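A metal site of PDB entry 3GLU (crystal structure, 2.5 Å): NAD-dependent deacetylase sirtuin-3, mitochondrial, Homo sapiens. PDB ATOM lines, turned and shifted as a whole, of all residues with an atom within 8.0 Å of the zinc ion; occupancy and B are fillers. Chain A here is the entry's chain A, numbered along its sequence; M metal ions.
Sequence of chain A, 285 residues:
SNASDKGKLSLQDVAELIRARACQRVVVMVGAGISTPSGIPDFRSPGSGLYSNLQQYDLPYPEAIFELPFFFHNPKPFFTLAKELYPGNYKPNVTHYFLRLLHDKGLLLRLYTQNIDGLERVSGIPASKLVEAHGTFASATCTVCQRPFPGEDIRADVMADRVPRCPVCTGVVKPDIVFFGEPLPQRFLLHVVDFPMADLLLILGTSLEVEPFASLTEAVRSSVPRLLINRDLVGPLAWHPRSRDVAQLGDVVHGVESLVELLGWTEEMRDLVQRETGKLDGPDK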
ATOM      1  N   THR A 141      -3.275  22.765  20.274  1.00  0.00           N
ATOM      2  CA  THR A 141      -3.316  21.964  19.081  1.00  0.00           C
ATOM      3  C   THR A 141      -4.741  21.981  18.543  1.00  0.00           C
ATOM      4  O   THR A 141      -5.718  21.811  19.324  1.00  0.00           O
ATOM      5  CB  THR A 141      -2.928  20.469  19.397  1.00  0.00           C
ATOM      6  OG1 THR A 141      -1.638  20.453  19.986  1.00  0.00           O
ATOM      7  CG2 THR A 141      -2.798  19.622  18.110  1.00  0.00           C
ATOM      8  N   CYS A 142      -4.889  22.189  17.234  1.00  0.00           N
ATOM      9  CA  CYS A 142      -6.231  22.074  16.645  1.00  0.00           C
ATOM     10  C   CYS A 142      -6.657  20.614  16.610  1.00  0.00           C
ATOM     11  O   CYS A 142      -5.918  19.742  16.170  1.00  0.00           O
ATOM     12  CB  CYS A 142      -6.289  22.651  15.247  1.00  0.00           C
ATOM     13  SG  CYS A 142      -7.810  22.129  14.434  1.00  0.00           S
ATOM     14  N   THR A 143      -7.849  20.341  17.145  1.00  0.00           N
ATOM     15  CA  THR A 143      -8.311  18.958  17.353  1.00  0.00           C
ATOM     16  C   THR A 143      -8.594  18.212  16.062  1.00  0.00           C
ATOM     17  O   THR A 143      -8.646  16.980  16.067  1.00  0.00           O
ATOM     18  CB  THR A 143      -9.587  18.895  18.166  1.00  0.00           C
ATOM     19  OG1 THR A 143     -10.580  19.739  17.560  1.00  0.00           O
ATOM     20  CG2 THR A 143      -9.306  19.225  19.705  1.00  0.00           C
ATOM     21  N   VAL A 144      -8.766  18.945  14.951  1.00  0.00           N
ATOM     22  CA  VAL A 144      -9.003  18.310  13.660  1.00  0.00           C
ATOM     23  C   VAL A 144      -7.740  18.188  12.765  1.00  0.00           C
ATOM     24  O   VAL A 144      -7.436  17.118  12.264  1.00  0.00           O
ATOM     25  CB  VAL A 144     -10.070  19.124  12.924  1.00  0.00           C
ATOM     26  CG1 VAL A 144     -10.260  18.629  11.489  1.00  0.00           C
ATOM     27  CG2 VAL A 144     -11.375  19.185  13.766  1.00  0.00           C
ATOM     28  N   CYS A 145      -6.973  19.274  12.577  1.00  0.00           N
ATOM     29  CA  CYS A 145      -5.853  19.208  11.628  1.00  0.00           C
ATOM     30  C   CYS A 145      -4.515  19.136  12.339  1.00  0.00           C
ATOM     31  O   CYS A 145      -3.439  19.151  11.682  1.00  0.00           O
ATOM     32  CB  CYS A 145      -5.861  20.404  10.675  1.00  0.00           C
ATOM     33  SG  CYS A 145      -5.496  22.010  11.502  1.00  0.00           S
ATOM     34  N   GLN A 146      -4.548  19.039  13.665  1.00  0.00           N
ATOM     35  CA  GLN A 146      -3.328  18.902  14.454  1.00  0.00           C
ATOM     36  C   GLN A 146      -2.342  20.032  14.184  1.00  0.00           C
ATOM     37  O   GLN A 146      -1.130  19.800  14.107  1.00  0.00           O
ATOM     38  CB  GLN A 146      -2.669  17.553  14.163  1.00  0.00           C
ATOM     39  CG  GLN A 146      -3.616  16.366  14.280  1.00  0.00           C
ATOM     40  CD  GLN A 146      -4.319  16.305  15.621  1.00  0.00           C
ATOM     41  OE1 GLN A 146      -3.766  16.699  16.647  1.00  0.00           O
ATOM     42  NE2 GLN A 146      -5.559  15.808  15.615  1.00  0.00           N
ATOM     43  N   ARG A 147      -2.860  21.245  14.058  1.00  0.00           N
ATOM     44  CA  ARG A 147      -2.000  22.406  13.839  1.00  0.00           C
ATOM     45  C   ARG A 147      -1.688  23.007  15.194  1.00  0.00           C
ATOM     46  O   ARG A 147      -2.602  23.299  15.967  1.00  0.00           O
ATOM     47  CB  ARG A 147      -2.690  23.422  12.942  1.00  0.00           C
ATOM     48  CG  ARG A 147      -2.300  23.341  11.484  1.00  0.00           C
ATOM     49  CD  ARG A 147      -2.977  24.438  10.665  1.00  0.00           C
ATOM     50  NE  ARG A 147      -2.667  24.320   9.239  1.00  0.00           N
ATOM     51  CZ  ARG A 147      -3.248  23.444   8.419  1.00  0.00           C
ATOM     52  NH1 ARG A 147      -2.904  23.411   7.144  1.00  0.00           N
ATOM     53  NH2 ARG A 147      -4.155  22.596   8.886  1.00  0.00           N
ATOM     54  N   PRO A 148      -0.412  23.170  15.497  1.00  0.00           N
ATOM     55  CA  PRO A 148      -0.006  23.689  16.830  1.00  0.00           C
ATOM     56  C   PRO A 148       0.000  25.232  16.931  1.00  0.00           C
ATOM     57  O   PRO A 148       0.306  25.908  15.974  1.00  0.00           O
ATOM     58  CB  PRO A 148       1.430  23.138  16.976  1.00  0.00           C
ATOM     59  CG  PRO A 148       1.986  23.255  15.541  1.00  0.00           C
ATOM     60  CD  PRO A 148       0.770  23.033  14.612  1.00  0.00           C
ATOM     61  N   PHE A 149      -0.350  25.790  18.093  1.00  0.00           N
ATOM     62  CA  PHE A 149      -0.404  27.248  18.272  1.00  0.00           C
ATOM     63  C   PHE A 149       0.200  27.599  19.622  1.00  0.00           C
ATOM     64  O   PHE A 149       0.092  26.817  20.594  1.00  0.00           O
ATOM     65  CB  PHE A 149      -1.862  27.776  18.215  1.00  0.00           C
ATOM     66  CG  PHE A 149      -2.561  27.519  16.906  1.00  0.00           C
ATOM     67  CD1 PHE A 149      -2.298  28.312  15.784  1.00  0.00           C
ATOM     68  CD2 PHE A 149      -3.496  26.483  16.784  1.00  0.00           C
ATOM     69  CE1 PHE A 149      -2.928  28.077  14.554  1.00  0.00           C
ATOM     70  CE2 PHE A 149      -4.134  26.241  15.594  1.00  0.00           C
ATOM     71  CZ  PHE A 149      -3.844  27.045  14.455  1.00  0.00           C
ATOM     72  N   ARG A 165     -11.379  28.566  17.894  1.00  0.00           N
ATOM     73  CA  ARG A 165     -11.526  27.809  16.663  1.00  0.00           C
ATOM     74  C   ARG A 165     -10.304  27.973  15.796  1.00  0.00           C
ATOM     75  O   ARG A 165      -9.654  28.983  15.788  1.00  0.00           O
ATOM     76  CB  ARG A 165     -12.701  28.373  15.906  1.00  0.00           C
ATOM     77  CG  ARG A 165     -14.025  28.156  16.651  1.00  0.00           C
ATOM     78  CD  ARG A 165     -14.639  26.926  16.059  1.00  0.00           C
ATOM     79  NE  ARG A 165     -15.474  26.261  17.032  1.00  0.00           N
ATOM     80  CZ  ARG A 165     -15.993  25.060  16.837  1.00  0.00           C
ATOM     81  NH1 ARG A 165     -15.740  24.397  15.739  1.00  0.00           N
ATOM     82  NH2 ARG A 165     -16.714  24.505  17.779  1.00  0.00           N
ATOM     83  N   CYS A 166     -10.005  26.943  15.009  1.00  0.00           N
ATOM     84  CA  CYS A 166      -8.832  26.955  14.143  1.00  0.00           C
ATOM     85  C   CYS A 166      -8.948  27.963  12.964  1.00  0.00           C
ATOM     86  O   CYS A 166      -9.972  28.019  12.309  1.00  0.00           O
ATOM     87  CB  CYS A 166      -8.503  25.552  13.686  1.00  0.00           C
ATOM     88  SG  CYS A 166      -7.098  25.540  12.582  1.00  0.00           S
ATOM     89  N   PRO A 167      -7.900  28.780  12.741  1.00  0.00           N
ATOM     90  CA  PRO A 167      -7.960  29.782  11.662  1.00  0.00           C
ATOM     91  C   PRO A 167      -7.833  29.145  10.281  1.00  0.00           C
ATOM     92  O   PRO A 167      -8.168  29.795   9.294  1.00  0.00           O
ATOM     93  CB  PRO A 167      -6.729  30.683  11.925  1.00  0.00           C
ATOM     94  CG  PRO A 167      -6.203  30.314  13.337  1.00  0.00           C
ATOM     95  CD  PRO A 167      -6.648  28.873  13.521  1.00  0.00           C
ATOM     96  N   VAL A 168      -7.339  27.894  10.223  1.00  0.00           N
ATOM     97  CA  VAL A 168      -7.221  27.209   8.934  1.00  0.00           C
ATOM     98  C   VAL A 168      -8.410  26.251   8.629  1.00  0.00           C
ATOM     99  O   VAL A 168      -8.984  26.314   7.512  1.00  0.00           O
ATOM    100  CB  VAL A 168      -5.896  26.436   8.744  1.00  0.00           C
ATOM    101  CG1 VAL A 168      -5.934  25.758   7.383  1.00  0.00           C
ATOM    102  CG2 VAL A 168      -4.694  27.366   8.840  1.00  0.00           C
ATOM    103  N   CYS A 169      -8.811  25.416   9.603  1.00  0.00           N
ATOM    104  CA  CYS A 169      -9.901  24.448   9.323  1.00  0.00           C
ATOM    105  C   CYS A 169     -11.176  24.636  10.162  1.00  0.00           C
ATOM    106  O   CYS A 169     -12.108  23.872  10.024  1.00  0.00           O
ATOM    107  CB  CYS A 169      -9.424  22.996   9.497  1.00  0.00           C
ATOM    108  SG  CYS A 169      -9.414  22.523  11.207  1.00  0.00           S
ATOM    109  N   THR A 170     -11.190  25.660  11.010  1.00  0.00           N
ATOM    110  CA  THR A 170     -12.290  25.910  12.002  1.00  0.00           C
ATOM    111  C   THR A 170     -12.497  24.847  13.108  1.00  0.00           C
ATOM    112  O   THR A 170     -13.396  24.946  13.936  1.00  0.00           O
ATOM    113  CB  THR A 170     -13.659  26.065  11.322  1.00  0.00           C
ATOM    114  OG1 THR A 170     -14.047  24.786  10.817  1.00  0.00           O
ATOM    115  CG2 THR A 170     -13.661  27.153  10.185  1.00  0.00           C
ATOM    116  N   GLY A 171     -11.695  23.825  13.162  1.00  0.00           N
ATOM    117  CA  GLY A 171     -11.828  22.928  14.329  1.00  0.00           C
ATOM    118  C   GLY A 171     -11.577  23.653  15.648  1.00  0.00           C
ATOM    119  O   GLY A 171     -11.074  24.784  15.673  1.00  0.00           O
ATOM    120  N   VAL A 172     -11.987  23.012  16.730  1.00  0.00           N
ATOM    121  CA  VAL A 172     -11.792  23.514  18.084  1.00  0.00           C
ATOM    122  C   VAL A 172     -10.342  23.298  18.476  1.00  0.00           C
ATOM    123  O   VAL A 172      -9.798  22.136  18.410  1.00  0.00           O
ATOM    124  CB  VAL A 172     -12.705  22.738  19.062  1.00  0.00           C
ATOM    125  CG1 VAL A 172     -12.263  22.942  20.540  1.00  0.00           C
ATOM    126  CG2 VAL A 172     -14.209  23.089  18.807  1.00  0.00           C
ATOM    127  N   VAL A 173      -9.688  24.406  18.837  1.00  0.00           N
ATOM    128  CA  VAL A 173      -8.302  24.358  19.301  1.00  0.00           C
ATOM    129  C   VAL A 173      -8.258  24.018  20.794  1.00  0.00           C
ATOM    130  O   VAL A 173      -8.872  24.666  21.599  1.00  0.00           O
ATOM    131  CB  VAL A 173      -7.536  25.663  19.029  1.00  0.00           C
ATOM    132  CG1 VAL A 173      -6.184  25.618  19.639  1.00  0.00           C
ATOM    133  CG2 VAL A 173      -7.458  25.911  17.518  1.00  0.00           C
HETATM  134 ZN    ZN M   1      -7.389  23.151  12.257  1.00  0.00          ZN
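Four residues have an atom within 4 Å of the zinc ion: Cys 142, Cys 145, Cys 166 and Cys 169.
SG of Cys 145 is bound to the zinc ion.
The zinc ion is bound by SG of Cys 169 (2.4 Å).
SG of Cys 166 binds the zinc ion.
The zinc ion is bound by SG of Cys 142 (2.4 Å).
The zinc ion has four donor atoms within binding distance.
The side-chain sulfur (SG) of Cys 145 sits close to the guanidinium group (NH2) of Arg 147 (3.0 Å).
The side-chain sulfur (SG) of Cys 169 sits close to the backbone NH (N) of Gly 171 (3.3 Å).
The backbone NH of Cys 166 lies within hydrogen-bond range of the backbone carbonyl oxygen of Gly 171 (2.5 Å).
N of Val 168 lies close to SG of Cys 166 (3.3 Å).
O of Arg 147 sits at hydrogen-bond distance from N of Cys 142, at 2.8 Å.
The backbone NH (N) of Val 144 sits close to the side-chain sulfur (SG) of Cys 142 (3.4 Å).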
